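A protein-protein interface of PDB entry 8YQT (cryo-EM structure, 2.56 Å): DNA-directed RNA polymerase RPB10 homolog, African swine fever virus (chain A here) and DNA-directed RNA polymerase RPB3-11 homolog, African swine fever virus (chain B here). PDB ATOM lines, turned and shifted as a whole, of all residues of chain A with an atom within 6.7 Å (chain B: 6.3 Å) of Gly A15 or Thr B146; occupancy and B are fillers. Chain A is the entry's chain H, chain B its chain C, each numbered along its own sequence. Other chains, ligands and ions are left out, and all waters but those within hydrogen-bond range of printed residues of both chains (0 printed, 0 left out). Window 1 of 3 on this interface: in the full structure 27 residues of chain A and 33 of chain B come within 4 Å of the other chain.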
ATOM      1  N   ILE A   3      19.636  26.661   9.204  1.00  0.00           N
ATOM      2  CA  ILE A   3      18.619  25.870   9.906  1.00  0.00           C
ATOM      3  C   ILE A   3      17.619  26.825  10.544  1.00  0.00           C
ATOM      4  O   ILE A   3      18.030  27.793  11.212  1.00  0.00           O
ATOM      5  CB  ILE A   3      19.270  24.960  10.964  1.00  0.00           C
ATOM      6  CG1 ILE A   3      20.051  23.831  10.293  1.00  0.00           C
ATOM      7  CG2 ILE A   3      18.224  24.379  11.899  1.00  0.00           C
ATOM      8  CD1 ILE A   3      20.856  22.991  11.257  1.00  0.00           C
ATOM      9  N   PRO A   4      16.316  26.618  10.371  1.00  0.00           N
ATOM     10  CA  PRO A   4      15.341  27.608  10.842  1.00  0.00           C
ATOM     11  C   PRO A   4      15.390  27.795  12.350  1.00  0.00           C
ATOM     12  O   PRO A   4      15.788  26.910  13.109  1.00  0.00           O
ATOM     13  CB  PRO A   4      14.000  27.015  10.400  1.00  0.00           C
ATOM     14  CG  PRO A   4      14.265  25.559  10.249  1.00  0.00           C
ATOM     15  CD  PRO A   4      15.658  25.472   9.726  1.00  0.00           C
ATOM     16  N   VAL A   5      14.996  28.997  12.772  1.00  0.00           N
ATOM     17  CA  VAL A   5      14.982  29.331  14.192  1.00  0.00           C
ATOM     18  C   VAL A   5      14.008  28.431  14.938  1.00  0.00           C
ATOM     19  O   VAL A   5      14.303  27.932  16.029  1.00  0.00           O
ATOM     20  CB  VAL A   5      14.638  30.820  14.383  1.00  0.00           C
ATOM     21  CG1 VAL A   5      14.551  31.164  15.852  1.00  0.00           C
ATOM     22  CG2 VAL A   5      15.670  31.682  13.702  1.00  0.00           C
ATOM     23  N   VAL A   6      12.832  28.209  14.360  1.00  0.00           N
ATOM     24  CA  VAL A   6      11.844  27.299  14.911  1.00  0.00           C
ATOM     25  C   VAL A   6      11.454  26.309  13.825  1.00  0.00           C
ATOM     26  O   VAL A   6      11.654  26.547  12.633  1.00  0.00           O
ATOM     27  CB  VAL A   6      10.599  28.034  15.452  1.00  0.00           C
ATOM     28  CG1 VAL A   6      10.974  28.937  16.608  1.00  0.00           C
ATOM     29  CG2 VAL A   6       9.927  28.822  14.348  1.00  0.00           C
ATOM     30  N   CYS A   7      10.906  25.178  14.255  1.00  0.00           N
ATOM     31  CA  CYS A   7      10.395  24.195  13.314  1.00  0.00           C
ATOM     32  C   CYS A   7       9.310  24.815  12.443  1.00  0.00           C
ATOM     33  O   CYS A   7       8.412  25.499  12.938  1.00  0.00           O
ATOM     34  CB  CYS A   7       9.853  22.987  14.074  1.00  0.00           C
ATOM     35  SG  CYS A   7       8.994  21.777  13.071  1.00  0.00           S
ATOM     36  N   PHE A  12       8.531  24.552  17.424  1.00  0.00           N
ATOM     37  CA  PHE A  12       9.455  24.261  18.507  1.00  0.00           C
ATOM     38  C   PHE A  12      10.799  24.935  18.235  1.00  0.00           C
ATOM     39  O   PHE A  12      11.268  24.944  17.095  1.00  0.00           O
ATOM     40  CB  PHE A  12       9.639  22.751  18.663  1.00  0.00           C
ATOM     41  CG  PHE A  12      10.535  22.361  19.803  1.00  0.00           C
ATOM     42  CD1 PHE A  12      10.040  22.272  21.091  1.00  0.00           C
ATOM     43  CD2 PHE A  12      11.875  22.089  19.586  1.00  0.00           C
ATOM     44  CE1 PHE A  12      10.862  21.921  22.137  1.00  0.00           C
ATOM     45  CE2 PHE A  12      12.698  21.740  20.630  1.00  0.00           C
ATOM     46  CZ  PHE A  12      12.191  21.654  21.907  1.00  0.00           C
ATOM     47  N   PRO A  13      11.449  25.498  19.260  1.00  0.00           N
ATOM     48  CA  PRO A  13      12.701  26.229  19.026  1.00  0.00           C
ATOM     49  C   PRO A  13      13.843  25.322  18.601  1.00  0.00           C
ATOM     50  O   PRO A  13      14.725  24.988  19.393  1.00  0.00           O
ATOM     51  CB  PRO A  13      12.981  26.884  20.384  1.00  0.00           C
ATOM     52  CG  PRO A  13      12.255  26.044  21.359  1.00  0.00           C
ATOM     53  CD  PRO A  13      11.021  25.584  20.664  1.00  0.00           C
ATOM     54  N   ILE A  14      13.817  24.913  17.334  1.00  0.00           N
ATOM     55  CA  ILE A  14      14.855  24.046  16.784  1.00  0.00           C
ATOM     56  C   ILE A  14      16.194  24.768  16.703  1.00  0.00           C
ATOM     57  O   ILE A  14      17.249  24.160  16.912  1.00  0.00           O
ATOM     58  CB  ILE A  14      14.389  23.513  15.413  1.00  0.00           C
ATOM     59  CG1 ILE A  14      13.570  22.238  15.595  1.00  0.00           C
ATOM     60  CG2 ILE A  14      15.543  23.292  14.466  1.00  0.00           C
ATOM     61  CD1 ILE A  14      14.299  21.166  16.337  1.00  0.00           C
ATOM     62  N   GLY A  15      16.176  26.073  16.427  1.00  0.00           N
ATOM     63  CA  GLY A  15      17.400  26.777  16.087  1.00  0.00           C
ATOM     64  C   GLY A  15      18.381  26.939  17.231  1.00  0.00           C
ATOM     65  O   GLY A  15      19.587  27.059  16.998  1.00  0.00           O
ATOM     66  N   THR A  16      17.894  26.950  18.474  1.00  0.00           N
ATOM     67  CA  THR A  16      18.796  27.159  19.602  1.00  0.00           C
ATOM     68  C   THR A  16      19.800  26.029  19.760  1.00  0.00           C
ATOM     69  O   THR A  16      20.840  26.227  20.395  1.00  0.00           O
ATOM     70  CB  THR A  16      18.010  27.336  20.900  1.00  0.00           C
ATOM     71  OG1 THR A  16      18.910  27.297  22.013  1.00  0.00           O
ATOM     72  CG2 THR A  16      16.993  26.247  21.053  1.00  0.00           C
ATOM     73  N   TYR A  17      19.518  24.857  19.201  1.00  0.00           N
ATOM     74  CA  TYR A  17      20.458  23.748  19.194  1.00  0.00           C
ATOM     75  C   TYR A  17      21.043  23.500  17.814  1.00  0.00           C
ATOM     76  O   TYR A  17      21.723  22.491  17.617  1.00  0.00           O
ATOM     77  CB  TYR A  17      19.780  22.476  19.701  1.00  0.00           C
ATOM     78  CG  TYR A  17      18.845  22.711  20.855  1.00  0.00           C
ATOM     79  CD1 TYR A  17      19.334  22.983  22.120  1.00  0.00           C
ATOM     80  CD2 TYR A  17      17.472  22.661  20.678  1.00  0.00           C
ATOM     81  CE1 TYR A  17      18.486  23.203  23.175  1.00  0.00           C
ATOM     82  CE2 TYR A  17      16.615  22.877  21.731  1.00  0.00           C
ATOM     83  CZ  TYR A  17      17.128  23.149  22.977  1.00  0.00           C
ATOM     84  OH  TYR A  17      16.279  23.367  24.033  1.00  0.00           O
ATOM     85  N   ALA A  18      20.795  24.394  16.855  1.00  0.00           N
ATOM     86  CA  ALA A  18      21.226  24.149  15.485  1.00  0.00           C
ATOM     87  C   ALA A  18      22.743  24.151  15.366  1.00  0.00           C
ATOM     88  O   ALA A  18      23.338  23.160  14.925  1.00  0.00           O
ATOM     89  CB  ALA A  18      20.617  25.191  14.549  1.00  0.00           C
ATOM     90  N   ALA A  19      23.382  25.246  15.786  1.00  0.00           N
ATOM     91  CA  ALA A  19      24.825  25.385  15.623  1.00  0.00           C
ATOM     92  C   ALA A  19      25.562  24.198  16.223  1.00  0.00           C
ATOM     93  O   ALA A  19      26.344  23.528  15.535  1.00  0.00           O
ATOM     94  CB  ALA A  19      25.296  26.692  16.256  1.00  0.00           C
ATOM     95  N   ILE A  20      25.272  23.881  17.487  1.00  0.00           N
ATOM     96  CA  ILE A  20      25.879  22.713  18.119  1.00  0.00           C
ATOM     97  C   ILE A  20      25.609  21.471  17.284  1.00  0.00           C
ATOM     98  O   ILE A  20      26.540  20.760  16.876  1.00  0.00           O
ATOM     99  CB  ILE A  20      25.350  22.548  19.555  1.00  0.00           C
ATOM    100  CG1 ILE A  20      25.591  23.819  20.366  1.00  0.00           C
ATOM    101  CG2 ILE A  20      25.998  21.356  20.232  1.00  0.00           C
ATOM    102  CD1 ILE A  20      24.794  23.884  21.642  1.00  0.00           C
ATOM    103  N   LEU A  70      15.511  19.810  11.161  1.00  0.00           N
ATOM    104  CA  LEU A  70      16.874  19.930  11.660  1.00  0.00           C
ATOM    105  C   LEU A  70      17.852  19.169  10.773  1.00  0.00           C
ATOM    106  O   LEU A  70      18.934  19.670  10.449  1.00  0.00           O
ATOM    107  CB  LEU A  70      16.937  19.418  13.096  1.00  0.00           C
ATOM    108  CG  LEU A  70      18.243  19.605  13.854  1.00  0.00           C
ATOM    109  CD1 LEU A  70      18.393  21.034  14.324  1.00  0.00           C
ATOM    110  CD2 LEU A  70      18.297  18.643  15.017  1.00  0.00           C
ATOM    111  N   PHE B  30      30.303  27.726  22.095  1.00  0.00           N
ATOM    112  CA  PHE B  30      29.768  28.762  22.970  1.00  0.00           C
ATOM    113  C   PHE B  30      30.409  28.764  24.350  1.00  0.00           C
ATOM    114  O   PHE B  30      29.941  29.495  25.231  1.00  0.00           O
ATOM    115  CB  PHE B  30      28.250  28.608  23.107  1.00  0.00           C
ATOM    116  CG  PHE B  30      27.521  28.625  21.797  1.00  0.00           C
ATOM    117  CD1 PHE B  30      27.327  29.813  21.115  1.00  0.00           C
ATOM    118  CD2 PHE B  30      27.026  27.457  21.247  1.00  0.00           C
ATOM    119  CE1 PHE B  30      26.659  29.832  19.911  1.00  0.00           C
ATOM    120  CE2 PHE B  30      26.356  27.472  20.042  1.00  0.00           C
ATOM    121  CZ  PHE B  30      26.173  28.662  19.374  1.00  0.00           C
ATOM    122  N   LEU B  32      30.158  26.474  26.467  1.00  0.00           N
ATOM    123  CA  LEU B  32      28.946  26.114  27.190  1.00  0.00           C
ATOM    124  C   LEU B  32      29.137  24.768  27.872  1.00  0.00           C
ATOM    125  O   LEU B  32      29.392  23.759  27.206  1.00  0.00           O
ATOM    126  CB  LEU B  32      27.751  26.066  26.240  1.00  0.00           C
ATOM    127  CG  LEU B  32      26.398  25.665  26.826  1.00  0.00           C
ATOM    128  CD1 LEU B  32      25.914  26.701  27.820  1.00  0.00           C
ATOM    129  CD2 LEU B  32      25.380  25.461  25.721  1.00  0.00           C
ATOM    130  N   LEU B  36      21.199  25.902  29.231  1.00  0.00           N
ATOM    131  CA  LEU B  36      20.898  27.225  28.720  1.00  0.00           C
ATOM    132  C   LEU B  36      19.994  27.974  29.697  1.00  0.00           C
ATOM    133  O   LEU B  36      19.284  27.358  30.495  1.00  0.00           O
ATOM    134  CB  LEU B  36      20.241  27.119  27.348  1.00  0.00           C
ATOM    135  CG  LEU B  36      21.185  26.711  26.216  1.00  0.00           C
ATOM    136  CD1 LEU B  36      20.416  26.394  24.948  1.00  0.00           C
ATOM    137  CD2 LEU B  36      22.202  27.804  25.965  1.00  0.00           C
ATOM    138  N   ARG B  96      14.016  35.769  10.885  1.00  0.00           N
ATOM    139  CA  ARG B  96      14.768  35.049  11.910  1.00  0.00           C
ATOM    140  C   ARG B  96      14.506  35.632  13.294  1.00  0.00           C
ATOM    141  O   ARG B  96      14.250  34.894  14.251  1.00  0.00           O
ATOM    142  CB  ARG B  96      16.267  35.077  11.608  1.00  0.00           C
ATOM    143  CG  ARG B  96      16.671  34.615  10.225  1.00  0.00           C
ATOM    144  CD  ARG B  96      16.735  33.115  10.130  1.00  0.00           C
ATOM    145  NE  ARG B  96      17.753  32.538  10.997  1.00  0.00           N
ATOM    146  CZ  ARG B  96      18.097  31.259  10.988  1.00  0.00           C
ATOM    147  NH1 ARG B  96      17.531  30.397  10.163  1.00  0.00           N
ATOM    148  NH2 ARG B  96      19.026  30.833  11.837  1.00  0.00           N
ATOM    149  N   TYR B 126      25.316  35.467  16.065  1.00  0.00           N
ATOM    150  CA  TYR B 126      24.502  34.730  17.018  1.00  0.00           C
ATOM    151  C   TYR B 126      23.640  35.693  17.827  1.00  0.00           C
ATOM    152  O   TYR B 126      23.738  36.916  17.701  1.00  0.00           O
ATOM    153  CB  TYR B 126      25.378  33.893  17.950  1.00  0.00           C
ATOM    154  CG  TYR B 126      26.211  32.851  17.251  1.00  0.00           C
ATOM    155  CD1 TYR B 126      25.624  31.723  16.697  1.00  0.00           C
ATOM    156  CD2 TYR B 126      27.586  32.990  17.152  1.00  0.00           C
ATOM    157  CE1 TYR B 126      26.383  30.770  16.058  1.00  0.00           C
ATOM    158  CE2 TYR B 126      28.351  32.041  16.518  1.00  0.00           C
ATOM    159  CZ  TYR B 126      27.746  30.934  15.972  1.00  0.00           C
ATOM    160  OH  TYR B 126      28.511  29.985  15.338  1.00  0.00           O
ATOM    161  N   SER B 127      22.789  35.124  18.679  1.00  0.00           N
ATOM    162  CA  SER B 127      21.938  35.921  19.550  1.00  0.00           C
ATOM    163  C   SER B 127      22.693  36.549  20.711  1.00  0.00           C
ATOM    164  O   SER B 127      22.176  37.486  21.327  1.00  0.00           O
ATOM    165  CB  SER B 127      20.794  35.071  20.096  1.00  0.00           C
ATOM    166  OG  SER B 127      19.778  34.919  19.129  1.00  0.00           O
ATOM    167  N   ARG B 128      23.886  36.058  21.033  1.00  0.00           N
ATOM    168  CA  ARG B 128      24.709  36.700  22.047  1.00  0.00           C
ATOM    169  C   ARG B 128      25.247  38.047  21.593  1.00  0.00           C
ATOM    170  O   ARG B 128      25.775  38.797  22.419  1.00  0.00           O
ATOM    171  CB  ARG B 128      25.871  35.787  22.434  1.00  0.00           C
ATOM    172  CG  ARG B 128      26.785  35.448  21.281  1.00  0.00           C
ATOM    173  CD  ARG B 128      27.899  34.527  21.718  1.00  0.00           C
ATOM    174  NE  ARG B 128      28.755  34.158  20.600  1.00  0.00           N
ATOM    175  CZ  ARG B 128      29.787  33.330  20.689  1.00  0.00           C
ATOM    176  NH1 ARG B 128      30.124  32.771  21.839  1.00  0.00           N
ATOM    177  NH2 ARG B 128      30.494  33.057  19.598  1.00  0.00           N
ATOM    178  N   ASN B 144      17.793  32.804  24.507  1.00  0.00           N
ATOM    179  CA  ASN B 144      19.028  32.036  24.505  1.00  0.00           C
ATOM    180  C   ASN B 144      20.057  32.669  23.570  1.00  0.00           C
ATOM    181  O   ASN B 144      19.698  33.281  22.562  1.00  0.00           O
ATOM    182  CB  ASN B 144      18.759  30.600  24.077  1.00  0.00           C
ATOM    183  CG  ASN B 144      18.109  29.785  25.165  1.00  0.00           C
ATOM    184  OD1 ASN B 144      18.517  29.843  26.321  1.00  0.00           O
ATOM    185  ND2 ASN B 144      17.091  29.018  24.804  1.00  0.00           N
ATOM    186  N   PRO B 145      21.343  32.540  23.887  1.00  0.00           N
ATOM    187  CA  PRO B 145      22.374  33.173  23.055  1.00  0.00           C
ATOM    188  C   PRO B 145      22.909  32.289  21.937  1.00  0.00           C
ATOM    189  O   PRO B 145      23.939  32.610  21.339  1.00  0.00           O
ATOM    190  CB  PRO B 145      23.471  33.492  24.073  1.00  0.00           C
ATOM    191  CG  PRO B 145      23.361  32.388  25.057  1.00  0.00           C
ATOM    192  CD  PRO B 145      21.901  32.023  25.147  1.00  0.00           C
ATOM    193  N   THR B 146      22.234  31.181  21.639  1.00  0.00           N
ATOM    194  CA  THR B 146      22.765  30.182  20.721  1.00  0.00           C
ATOM    195  C   THR B 146      22.031  30.147  19.384  1.00  0.00           C
ATOM    196  O   THR B 146      22.156  29.166  18.644  1.00  0.00           O
ATOM    197  CB  THR B 146      22.737  28.800  21.371  1.00  0.00           C
ATOM    198  OG1 THR B 146      21.400  28.486  21.773  1.00  0.00           O
ATOM    199  CG2 THR B 146      23.643  28.763  22.583  1.00  0.00           C
ATOM    200  N   PHE B 147      21.274  31.187  19.053  1.00  0.00           N
ATOM    201  CA  PHE B 147      20.547  31.237  17.791  1.00  0.00           C
ATOM    202  C   PHE B 147      21.431  31.821  16.701  1.00  0.00           C
ATOM    203  O   PHE B 147      22.012  32.893  16.880  1.00  0.00           O
ATOM    204  CB  PHE B 147      19.275  32.074  17.923  1.00  0.00           C
ATOM    205  CG  PHE B 147      18.193  31.423  18.727  1.00  0.00           C
ATOM    206  CD1 PHE B 147      17.275  30.588  18.124  1.00  0.00           C
ATOM    207  CD2 PHE B 147      18.086  31.661  20.084  1.00  0.00           C
ATOM    208  CE1 PHE B 147      16.276  29.996  18.857  1.00  0.00           C
ATOM    209  CE2 PHE B 147      17.089  31.072  20.821  1.00  0.00           C
ATOM    210  CZ  PHE B 147      16.182  30.239  20.207  1.00  0.00           C
ATOM    211  N   GLU B 148      21.519  31.125  15.571  1.00  0.00           N
ATOM    212  CA  GLU B 148      22.240  31.630  14.405  1.00  0.00           C
ATOM    213  C   GLU B 148      21.368  32.671  13.721  1.00  0.00           C
ATOM    214  O   GLU B 148      20.480  32.334  12.938  1.00  0.00           O
ATOM    215  CB  GLU B 148      22.579  30.500  13.442  1.00  0.00           C
ATOM    216  CG  GLU B 148      23.628  29.524  13.921  1.00  0.00           C
ATOM    217  CD  GLU B 148      23.697  28.297  13.033  1.00  0.00           C
ATOM    218  OE1 GLU B 148      22.734  28.060  12.277  1.00  0.00           O
ATOM    219  OE2 GLU B 148      24.714  27.578  13.080  1.00  0.00           O
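NH1 of Arg B96 lies within hydrogen-bond range of O of Ile A3 (2.9 Å). The side-chain hydroxyl (OG1) of Thr B146 lies within hydrogen-bond range of the backbone carbonyl oxygen (O) of Thr A16, at 2.7 Å.
The guanidinium group of Arg B96 sits close to the backbone carbonyl oxygen of Glu B148 (3.4 Å). The backbone NH (N) of Ser B127 sits at hydrogen-bond distance from the backbone carbonyl oxygen (O) of Phe B147 (3.0 Å). O of Val A5 lies within hydrogen-bond range of N of Gly A15, 2.7 Å away. O of Pro A4 lies close to N of Gly A15, 3.4 Å away. The backbone carbonyl oxygen of Val A5 is in hydrogen-bond range of the backbone NH of Ile A14, at 3.3 Å.
Pro A4 touches Arg B96. Arg B96 touches Val A5 (NE to CG2, 3.5 Å). CG1 of Val A5 touches CD1 of Phe B147, 3.6 Å away. O of Thr B146 touches O of Gly A15, at 3.7 Å. Gly A15 touches Phe B147. Asn B144 touches Thr A16 (ND2 to OG1, 3.7 Å). N of Thr A16 touches CE1 of Phe B147 (3.5 Å). Ala A19 touches Phe B30. Glu B148 touches Ala A19. CE2 of Phe B30 touches CG1 of Ile A20, at 3.7 Å.
Of the printed residues of chain B, Ile A3 touches Arg B96 (2.9 Å). Of chain B, only Thr B146 and Phe B147 come within 4 Å of Gly A15. Printed residues of chain B within 4 Å of Thr A16: Leu B36 (3.4 Å), Asn B144 (3.7 Å), Thr B146 (2.7 Å) and Phe B147 (3.5 Å). Printed residues of chain B within 4 Å of Ala A19: Phe B30 (3.8 Å) and Glu B148 (3.3 Å). Printed residues of chain A within 4 Å of Arg B96: Ile A3 (2.9 Å), Pro A4 (3.6 Å) and Val A5 (3.5 Å). Ser B127 touches none of the printed residues of chain A. Of the printed residues of chain A, Asn B144 touches Thr A16. Of chain A, only Gly A15 and Thr A16 come within 4 Å of Thr B146. The nearest printed residue of chain A that does not touch Asn B144 is Tyr A17 (5.8 Å).
Printed residues of chain A that touch a printed residue of chain B: Ile A3, Pro A4, Val A5, Gly A15, Thr A16, Ala A19 and Ile A20. Of the 12 printed residues of chain B, 7 touch a printed residue of chain A. Hydrophobic or aromatic side chains of chain B within 4 Å of the printed part of chain A: Phe B30, Leu B36 and Phe B147. Among the printed residues, no Asp or Glu carboxylate lies within 4 Å of a Lys or Arg side-chain nitrogen of the other chain.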
